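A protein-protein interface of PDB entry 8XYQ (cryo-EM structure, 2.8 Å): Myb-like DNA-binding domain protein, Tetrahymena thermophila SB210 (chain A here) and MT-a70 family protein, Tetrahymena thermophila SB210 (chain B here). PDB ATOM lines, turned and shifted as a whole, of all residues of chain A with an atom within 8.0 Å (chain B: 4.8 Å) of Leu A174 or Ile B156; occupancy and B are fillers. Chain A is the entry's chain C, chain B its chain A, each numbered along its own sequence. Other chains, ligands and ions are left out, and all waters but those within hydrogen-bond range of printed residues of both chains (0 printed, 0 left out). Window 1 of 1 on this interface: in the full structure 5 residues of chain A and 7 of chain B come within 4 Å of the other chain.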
ATOM      1  N   LEU A 157       7.740  18.790 -24.233  1.00  0.00           N
ATOM      2  CA  LEU A 157       6.713  18.145 -23.428  1.00  0.00           C
ATOM      3  C   LEU A 157       5.337  18.203 -24.087  1.00  0.00           C
ATOM      4  O   LEU A 157       4.370  17.674 -23.532  1.00  0.00           O
ATOM      5  CB  LEU A 157       6.680  18.805 -22.037  1.00  0.00           C
ATOM      6  CG  LEU A 157       5.852  18.315 -20.842  1.00  0.00           C
ATOM      7  CD1 LEU A 157       6.293  16.931 -20.404  1.00  0.00           C
ATOM      8  CD2 LEU A 157       5.958  19.298 -19.689  1.00  0.00           C
ATOM      9  N   ASP A 159       4.025  16.807 -26.883  1.00  0.00           N
ATOM     10  CA  ASP A 159       3.462  15.541 -27.343  1.00  0.00           C
ATOM     11  C   ASP A 159       2.893  14.750 -26.173  1.00  0.00           C
ATOM     12  O   ASP A 159       1.858  14.090 -26.300  1.00  0.00           O
ATOM     13  CB  ASP A 159       4.514  14.717 -28.090  1.00  0.00           C
ATOM     14  CG  ASP A 159       5.850  14.688 -27.379  1.00  0.00           C
ATOM     15  OD1 ASP A 159       6.429  15.772 -27.161  1.00  0.00           O
ATOM     16  OD2 ASP A 159       6.322  13.582 -27.042  1.00  0.00           O
ATOM     17  N   ILE A 160       3.572  14.811 -25.031  1.00  0.00           N
ATOM     18  CA  ILE A 160       3.106  14.182 -23.803  1.00  0.00           C
ATOM     19  C   ILE A 160       1.876  14.911 -23.277  1.00  0.00           C
ATOM     20  O   ILE A 160       0.947  14.290 -22.749  1.00  0.00           O
ATOM     21  CB  ILE A 160       4.225  14.163 -22.751  1.00  0.00           C
ATOM     22  CG1 ILE A 160       5.495  13.551 -23.346  1.00  0.00           C
ATOM     23  CG2 ILE A 160       3.771  13.400 -21.532  1.00  0.00           C
ATOM     24  CD1 ILE A 160       6.760  13.944 -22.623  1.00  0.00           C
ATOM     25  N   GLU A 161       1.859  16.236 -23.437  1.00  0.00           N
ATOM     26  CA  GLU A 161       0.875  17.116 -22.812  1.00  0.00           C
ATOM     27  C   GLU A 161      -0.546  16.862 -23.316  1.00  0.00           C
ATOM     28  O   GLU A 161      -1.519  17.298 -22.690  1.00  0.00           O
ATOM     29  CB  GLU A 161       1.293  18.573 -23.040  1.00  0.00           C
ATOM     30  CG  GLU A 161       0.554  19.615 -22.212  1.00  0.00           C
ATOM     31  CD  GLU A 161       1.039  21.024 -22.488  1.00  0.00           C
ATOM     32  OE1 GLU A 161       2.249  21.281 -22.307  1.00  0.00           O
ATOM     33  OE2 GLU A 161       0.216  21.874 -22.888  1.00  0.00           O
ATOM     34  N   ASN A 167      -2.437   6.607 -20.139  1.00  0.00           N
ATOM     35  CA  ASN A 167      -1.373   6.703 -19.145  1.00  0.00           C
ATOM     36  C   ASN A 167      -0.162   5.837 -19.466  1.00  0.00           C
ATOM     37  O   ASN A 167       0.895   6.043 -18.861  1.00  0.00           O
ATOM     38  CB  ASN A 167      -1.917   6.330 -17.767  1.00  0.00           C
ATOM     39  CG  ASN A 167      -3.275   6.941 -17.494  1.00  0.00           C
ATOM     40  OD1 ASN A 167      -4.167   6.906 -18.342  1.00  0.00           O
ATOM     41  ND2 ASN A 167      -3.442   7.505 -16.305  1.00  0.00           N
ATOM     42  N   LEU A 168      -0.282   4.882 -20.389  1.00  0.00           N
ATOM     43  CA  LEU A 168       0.845   4.019 -20.725  1.00  0.00           C
ATOM     44  C   LEU A 168       1.686   4.583 -21.866  1.00  0.00           C
ATOM     45  O   LEU A 168       2.920   4.583 -21.786  1.00  0.00           O
ATOM     46  CB  LEU A 168       0.350   2.617 -21.083  1.00  0.00           C
ATOM     47  CG  LEU A 168       1.466   1.625 -21.410  1.00  0.00           C
ATOM     48  CD1 LEU A 168       2.410   1.461 -20.228  1.00  0.00           C
ATOM     49  CD2 LEU A 168       0.887   0.294 -21.840  1.00  0.00           C
ATOM     50  N   GLU A 169       1.044   5.061 -22.935  1.00  0.00           N
ATOM     51  CA  GLU A 169       1.800   5.683 -24.017  1.00  0.00           C
ATOM     52  C   GLU A 169       2.438   6.986 -23.552  1.00  0.00           C
ATOM     53  O   GLU A 169       3.547   7.329 -23.981  1.00  0.00           O
ATOM     54  CB  GLU A 169       0.908   5.925 -25.233  1.00  0.00           C
ATOM     55  CG  GLU A 169      -0.454   6.514 -24.927  1.00  0.00           C
ATOM     56  CD  GLU A 169      -1.535   5.956 -25.832  1.00  0.00           C
ATOM     57  OE1 GLU A 169      -2.709   6.345 -25.669  1.00  0.00           O
ATOM     58  OE2 GLU A 169      -1.210   5.123 -26.703  1.00  0.00           O
ATOM     59  N   ILE A 170       1.755   7.712 -22.661  1.00  0.00           N
ATOM     60  CA  ILE A 170       2.342   8.899 -22.040  1.00  0.00           C
ATOM     61  C   ILE A 170       3.620   8.527 -21.303  1.00  0.00           C
ATOM     62  O   ILE A 170       4.650   9.197 -21.436  1.00  0.00           O
ATOM     63  CB  ILE A 170       1.324   9.571 -21.099  1.00  0.00           C
ATOM     64  CG1 ILE A 170       0.327  10.414 -21.893  1.00  0.00           C
ATOM     65  CG2 ILE A 170       2.021  10.429 -20.057  1.00  0.00           C
ATOM     66  CD1 ILE A 170      -0.721  11.087 -21.029  1.00  0.00           C
ATOM     67  N   LEU A 171       3.583   7.425 -20.552  1.00  0.00           N
ATOM     68  CA  LEU A 171       4.728   7.054 -19.730  1.00  0.00           C
ATOM     69  C   LEU A 171       5.870   6.523 -20.593  1.00  0.00           C
ATOM     70  O   LEU A 171       7.049   6.748 -20.287  1.00  0.00           O
ATOM     71  CB  LEU A 171       4.278   6.048 -18.668  1.00  0.00           C
ATOM     72  CG  LEU A 171       5.000   5.990 -17.316  1.00  0.00           C
ATOM     73  CD1 LEU A 171       4.141   5.240 -16.317  1.00  0.00           C
ATOM     74  CD2 LEU A 171       6.355   5.345 -17.399  1.00  0.00           C
ATOM     75  N   THR A 172       5.535   5.855 -21.699  1.00  0.00           N
ATOM     76  CA  THR A 172       6.547   5.483 -22.686  1.00  0.00           C
ATOM     77  C   THR A 172       7.210   6.723 -23.280  1.00  0.00           C
ATOM     78  O   THR A 172       8.434   6.757 -23.463  1.00  0.00           O
ATOM     79  CB  THR A 172       5.912   4.613 -23.778  1.00  0.00           C
ATOM     80  OG1 THR A 172       5.736   3.277 -23.288  1.00  0.00           O
ATOM     81  CG2 THR A 172       6.775   4.564 -25.028  1.00  0.00           C
ATOM     82  N   HIS A 173       6.416   7.763 -23.560  1.00  0.00           N
ATOM     83  CA  HIS A 173       6.974   9.014 -24.068  1.00  0.00           C
ATOM     84  C   HIS A 173       7.886   9.680 -23.041  1.00  0.00           C
ATOM     85  O   HIS A 173       8.949  10.205 -23.396  1.00  0.00           O
ATOM     86  CB  HIS A 173       5.846   9.959 -24.478  1.00  0.00           C
ATOM     87  CG  HIS A 173       5.096   9.507 -25.692  1.00  0.00           C
ATOM     88  ND1 HIS A 173       5.664   8.707 -26.661  1.00  0.00           N
ATOM     89  CD2 HIS A 173       3.822   9.730 -26.090  1.00  0.00           C
ATOM     90  CE1 HIS A 173       4.774   8.462 -27.604  1.00  0.00           C
ATOM     91  NE2 HIS A 173       3.648   9.072 -27.282  1.00  0.00           N
ATOM     92  N   LEU A 174       7.486   9.677 -21.764  1.00  0.00           N
ATOM     93  CA  LEU A 174       8.340  10.256 -20.728  1.00  0.00           C
ATOM     94  C   LEU A 174       9.655   9.494 -20.603  1.00  0.00           C
ATOM     95  O   LEU A 174      10.716  10.112 -20.440  1.00  0.00           O
ATOM     96  CB  LEU A 174       7.630  10.289 -19.369  1.00  0.00           C
ATOM     97  CG  LEU A 174       6.169  10.735 -19.194  1.00  0.00           C
ATOM     98  CD1 LEU A 174       5.487  10.069 -18.006  1.00  0.00           C
ATOM     99  CD2 LEU A 174       6.046  12.219 -19.053  1.00  0.00           C
ATOM    100  N   TYR A 175       9.608   8.162 -20.701  1.00  0.00           N
ATOM    101  CA  TYR A 175      10.839   7.381 -20.602  1.00  0.00           C
ATOM    102  C   TYR A 175      11.731   7.573 -21.823  1.00  0.00           C
ATOM    103  O   TYR A 175      12.961   7.598 -21.695  1.00  0.00           O
ATOM    104  CB  TYR A 175      10.522   5.902 -20.397  1.00  0.00           C
ATOM    105  CG  TYR A 175      10.763   5.432 -18.982  1.00  0.00           C
ATOM    106  CD1 TYR A 175      12.046   5.409 -18.444  1.00  0.00           C
ATOM    107  CD2 TYR A 175       9.714   5.012 -18.188  1.00  0.00           C
ATOM    108  CE1 TYR A 175      12.269   4.977 -17.151  1.00  0.00           C
ATOM    109  CE2 TYR A 175       9.925   4.582 -16.896  1.00  0.00           C
ATOM    110  CZ  TYR A 175      11.204   4.566 -16.384  1.00  0.00           C
ATOM    111  OH  TYR A 175      11.423   4.139 -15.097  1.00  0.00           O
ATOM    112  N   ASN A 176      11.140   7.701 -23.015  1.00  0.00           N
ATOM    113  CA  ASN A 176      11.944   7.995 -24.200  1.00  0.00           C
ATOM    114  C   ASN A 176      12.589   9.371 -24.104  1.00  0.00           C
ATOM    115  O   ASN A 176      13.743   9.551 -24.525  1.00  0.00           O
ATOM    116  CB  ASN A 176      11.091   7.897 -25.465  1.00  0.00           C
ATOM    117  CG  ASN A 176      10.608   6.485 -25.734  1.00  0.00           C
ATOM    118  OD1 ASN A 176      11.333   5.516 -25.509  1.00  0.00           O
ATOM    119  ND2 ASN A 176       9.382   6.362 -26.228  1.00  0.00           N
ATOM    120  N   LEU A 177      11.861  10.349 -23.556  1.00  0.00           N
ATOM    121  CA  LEU A 177      12.448  11.661 -23.312  1.00  0.00           C
ATOM    122  C   LEU A 177      13.607  11.563 -22.329  1.00  0.00           C
ATOM    123  O   LEU A 177      14.649  12.199 -22.530  1.00  0.00           O
ATOM    124  CB  LEU A 177      11.377  12.631 -22.806  1.00  0.00           C
ATOM    125  CG  LEU A 177      11.655  14.134 -22.927  1.00  0.00           C
ATOM    126  CD1 LEU A 177      10.360  14.891 -23.167  1.00  0.00           C
ATOM    127  CD2 LEU A 177      12.357  14.690 -21.693  1.00  0.00           C
ATOM    128  N   LYS A 178      13.454  10.759 -21.269  1.00  0.00           N
ATOM    129  CA  LYS A 178      14.578  10.529 -20.365  1.00  0.00           C
ATOM    130  C   LYS A 178      15.770   9.903 -21.067  1.00  0.00           C
ATOM    131  O   LYS A 178      16.907  10.299 -20.796  1.00  0.00           O
ATOM    132  CB  LYS A 178      14.224   9.610 -19.198  1.00  0.00           C
ATOM    133  CG  LYS A 178      13.211  10.101 -18.211  1.00  0.00           C
ATOM    134  CD  LYS A 178      13.717   9.703 -16.832  1.00  0.00           C
ATOM    135  CE  LYS A 178      13.164   8.375 -16.360  1.00  0.00           C
ATOM    136  NZ  LYS A 178      14.007   7.771 -15.292  1.00  0.00           N
ATOM    137  N   ALA A 179      15.534   8.923 -21.939  1.00  0.00           N
ATOM    138  CA  ALA A 179      16.629   8.263 -22.640  1.00  0.00           C
ATOM    139  C   ALA A 179      17.391   9.241 -23.526  1.00  0.00           C
ATOM    140  O   ALA A 179      18.627   9.298 -23.481  1.00  0.00           O
ATOM    141  CB  ALA A 179      16.095   7.091 -23.465  1.00  0.00           C
ATOM    142  N   GLU A 180      16.671  10.054 -24.306  1.00  0.00           N
ATOM    143  CA  GLU A 180      17.368  10.970 -25.205  1.00  0.00           C
ATOM    144  C   GLU A 180      18.066  12.092 -24.438  1.00  0.00           C
ATOM    145  O   GLU A 180      19.214  12.438 -24.753  1.00  0.00           O
ATOM    146  CB  GLU A 180      16.414  11.526 -26.268  1.00  0.00           C
ATOM    147  CG  GLU A 180      15.184  12.248 -25.759  1.00  0.00           C
ATOM    148  CD  GLU A 180      14.093  12.324 -26.809  1.00  0.00           C
ATOM    149  OE1 GLU A 180      14.067  11.455 -27.705  1.00  0.00           O
ATOM    150  OE2 GLU A 180      13.263  13.256 -26.741  1.00  0.00           O
ATOM    151  N   ILE A 181      17.422  12.657 -23.411  1.00  0.00           N
ATOM    152  CA  ILE A 181      18.102  13.718 -22.672  1.00  0.00           C
ATOM    153  C   ILE A 181      19.221  13.182 -21.788  1.00  0.00           C
ATOM    154  O   ILE A 181      20.183  13.910 -21.527  1.00  0.00           O
ATOM    155  CB  ILE A 181      17.124  14.577 -21.848  1.00  0.00           C
ATOM    156  CG1 ILE A 181      16.664  13.857 -20.577  1.00  0.00           C
ATOM    157  CG2 ILE A 181      15.966  15.071 -22.714  1.00  0.00           C
ATOM    158  CD1 ILE A 181      16.156  14.792 -19.507  1.00  0.00           C
ATOM    159  N   ILE B 152      10.397  16.114 -15.185  1.00  0.00           N
ATOM    160  CA  ILE B 152       9.974  14.895 -15.860  1.00  0.00           C
ATOM    161  C   ILE B 152       9.948  13.738 -14.861  1.00  0.00           C
ATOM    162  O   ILE B 152       9.130  12.825 -14.993  1.00  0.00           O
ATOM    163  CB  ILE B 152      10.876  14.616 -17.084  1.00  0.00           C
ATOM    164  CG1 ILE B 152      10.140  13.797 -18.128  1.00  0.00           C
ATOM    165  CG2 ILE B 152      12.106  13.815 -16.740  1.00  0.00           C
ATOM    166  CD1 ILE B 152       8.777  14.316 -18.405  1.00  0.00           C
ATOM    167  N   GLU B 153      10.794  13.784 -13.824  1.00  0.00           N
ATOM    168  CA  GLU B 153      10.677  12.840 -12.714  1.00  0.00           C
ATOM    169  C   GLU B 153       9.357  13.025 -11.980  1.00  0.00           C
ATOM    170  O   GLU B 153       8.686  12.045 -11.630  1.00  0.00           O
ATOM    171  CB  GLU B 153      11.848  13.002 -11.742  1.00  0.00           C
ATOM    172  CG  GLU B 153      13.200  12.519 -12.248  1.00  0.00           C
ATOM    173  CD  GLU B 153      13.159  11.099 -12.766  1.00  0.00           C
ATOM    174  OE1 GLU B 153      13.363  10.162 -11.964  1.00  0.00           O
ATOM    175  OE2 GLU B 153      12.935  10.916 -13.977  1.00  0.00           O
ATOM    176  N   LYS B 154       8.972  14.280 -11.725  1.00  0.00           N
ATOM    177  CA  LYS B 154       7.684  14.524 -11.077  1.00  0.00           C
ATOM    178  C   LYS B 154       6.516  14.064 -11.945  1.00  0.00           C
ATOM    179  O   LYS B 154       5.551  13.480 -11.432  1.00  0.00           O
ATOM    180  CB  LYS B 154       7.538  16.003 -10.726  1.00  0.00           C
ATOM    181  CG  LYS B 154       8.635  16.540  -9.821  1.00  0.00           C
ATOM    182  CD  LYS B 154       8.603  15.870  -8.457  1.00  0.00           C
ATOM    183  CE  LYS B 154       9.904  15.141  -8.164  1.00  0.00           C
ATOM    184  NZ  LYS B 154       9.798  14.274  -6.957  1.00  0.00           N
ATOM    185  N   ARG B 155       6.594  14.304 -13.256  1.00  0.00           N
ATOM    186  CA  ARG B 155       5.550  13.852 -14.170  1.00  0.00           C
ATOM    187  C   ARG B 155       5.475  12.329 -14.209  1.00  0.00           C
ATOM    188  O   ARG B 155       4.382  11.750 -14.252  1.00  0.00           O
ATOM    189  CB  ARG B 155       5.795  14.417 -15.571  1.00  0.00           C
ATOM    190  CG  ARG B 155       5.182  15.792 -15.806  1.00  0.00           C
ATOM    191  CD  ARG B 155       3.668  15.707 -15.932  1.00  0.00           C
ATOM    192  NE  ARG B 155       3.011  16.894 -15.398  1.00  0.00           N
ATOM    193  CZ  ARG B 155       2.436  16.956 -14.205  1.00  0.00           C
ATOM    194  NH1 ARG B 155       2.420  15.916 -13.391  1.00  0.00           N
ATOM    195  NH2 ARG B 155       1.866  18.094 -13.817  1.00  0.00           N
ATOM    196  N   ILE B 156       6.634  11.664 -14.183  1.00  0.00           N
ATOM    197  CA  ILE B 156       6.672  10.207 -14.166  1.00  0.00           C
ATOM    198  C   ILE B 156       6.077   9.664 -12.877  1.00  0.00           C
ATOM    199  O   ILE B 156       5.348   8.671 -12.905  1.00  0.00           O
ATOM    200  CB  ILE B 156       8.114   9.718 -14.402  1.00  0.00           C
ATOM    201  CG1 ILE B 156       8.309   9.406 -15.882  1.00  0.00           C
ATOM    202  CG2 ILE B 156       8.457   8.492 -13.558  1.00  0.00           C
ATOM    203  CD1 ILE B 156       9.717   9.177 -16.274  1.00  0.00           C
ATOM    204  N   LEU B 157       6.352  10.304 -11.737  1.00  0.00           N
ATOM    205  CA  LEU B 157       5.757   9.861 -10.477  1.00  0.00           C
ATOM    206  C   LEU B 157       4.241  10.029 -10.496  1.00  0.00           C
ATOM    207  O   LEU B 157       3.497   9.141 -10.053  1.00  0.00           O
ATOM    208  CB  LEU B 157       6.373  10.629  -9.308  1.00  0.00           C
ATOM    209  CG  LEU B 157       7.384   9.873  -8.442  1.00  0.00           C
ATOM    210  CD1 LEU B 157       6.674   8.879  -7.536  1.00  0.00           C
ATOM    211  CD2 LEU B 157       8.428   9.171  -9.299  1.00  0.00           C
ATOM    212  N   HIS B 158       3.765  11.163 -11.024  1.00  0.00           N
ATOM    213  CA  HIS B 158       2.327  11.404 -11.106  1.00  0.00           C
ATOM    214  C   HIS B 158       1.639  10.379 -12.003  1.00  0.00           C
ATOM    215  O   HIS B 158       0.592   9.824 -11.640  1.00  0.00           O
ATOM    216  CB  HIS B 158       2.071  12.825 -11.612  1.00  0.00           C
ATOM    217  CG  HIS B 158       0.622  13.194 -11.686  1.00  0.00           C
ATOM    218  ND1 HIS B 158       0.099  13.951 -12.711  1.00  0.00           N
ATOM    219  CD2 HIS B 158      -0.412  12.913 -10.860  1.00  0.00           C
ATOM    220  CE1 HIS B 158      -1.196  14.122 -12.514  1.00  0.00           C
ATOM    221  NE2 HIS B 158      -1.532  13.501 -11.397  1.00  0.00           N
ATOM    222  N   TYR B 159       2.227  10.089 -13.165  1.00  0.00           N
ATOM    223  CA  TYR B 159       1.606   9.135 -14.077  1.00  0.00           C
ATOM    224  C   TYR B 159       1.783   7.696 -13.607  1.00  0.00           C
ATOM    225  O   TYR B 159       0.944   6.846 -13.915  1.00  0.00           O
ATOM    226  CB  TYR B 159       2.160   9.330 -15.487  1.00  0.00           C
ATOM    227  CG  TYR B 159       1.505  10.491 -16.201  1.00  0.00           C
ATOM    228  CD1 TYR B 159       0.137  10.493 -16.446  1.00  0.00           C
ATOM    229  CD2 TYR B 159       2.245  11.595 -16.603  1.00  0.00           C
ATOM    230  CE1 TYR B 159      -0.472  11.555 -17.086  1.00  0.00           C
ATOM    231  CE2 TYR B 159       1.645  12.662 -17.242  1.00  0.00           C
ATOM    232  CZ  TYR B 159       0.286  12.636 -17.481  1.00  0.00           C
ATOM    233  OH  TYR B 159      -0.318  13.695 -18.118  1.00  0.00           O
ATOM    234  N   LYS B 160       2.845   7.413 -12.850  1.00  0.00           N
ATOM    235  CA  LYS B 160       2.985   6.132 -12.167  1.00  0.00           C
ATOM    236  C   LYS B 160       1.839   5.914 -11.195  1.00  0.00           C
ATOM    237  O   LYS B 160       1.227   4.839 -11.163  1.00  0.00           O
ATOM    238  CB  LYS B 160       4.317   6.107 -11.416  1.00  0.00           C
ATOM    239  CG  LYS B 160       5.097   4.809 -11.430  1.00  0.00           C
ATOM    240  CD  LYS B 160       6.041   4.738 -12.612  1.00  0.00           C
ATOM    241  CE  LYS B 160       7.242   3.865 -12.282  1.00  0.00           C
ATOM    242  NZ  LYS B 160       6.885   2.445 -12.032  1.00  0.00           N
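Among the printed residues, pairs that only touch across the chains: Leu A174 with Ile B152 (3.5 Å), Lys A178 with Ile B156 (3.5 Å), Leu A174 with Ile B156 (3.6 Å), Ile A170 with Tyr B159 (3.6 Å) and Leu A174 with Tyr B159 (3.8 Å).
Of chain B, only Ile B152, Ile B156 and Tyr B159 come within 4 Å of Leu A174. Of the printed residues of chain A, Ile B156 touches Leu A174 and Lys A178. Printed residues of chain B within 4 Å of Ile A170: Tyr B159. Of the printed residues of chain A, Ile B152 touches Leu A174. Printed residues of chain B within 4 Å of Lys A178: Glu B153 (3.2 Å) and Ile B156 (3.5 Å). Printed residues of chain A within 4 Å of Glu B153: Lys A178 (3.2 Å). Printed residues of chain A within 4 Å of Tyr B159: Ile A170 and Leu A174. The nearest residue of chain B that does not touch Leu A174 is Arg B155 (4.1 Å). The nearest printed residue of chain B that does not touch Ile A170 is Arg B155 (6.4 Å).
OE2 of Glu B153 lies within salt-bridge range of NZ of Lys A178 (3.6 Å).
Of the 9 printed residues of chain B, 4 touch a printed residue of chain A. Of the 19 printed residues of chain A, 3 touch a printed residue of chain B. Printed residues of chain A that touch a printed residue of chain B: Ile A170, Leu A174 and Lys A178. Hydrophobic or aromatic side chains of chain A within 4 Å of the printed part of chain B: Ile A170 and Leu A174. Among the printed residues, Asp or Glu carboxylates within 4 Å of a Lys or Arg side-chain nitrogen of the other chain: Lys A178 with Glu B153.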
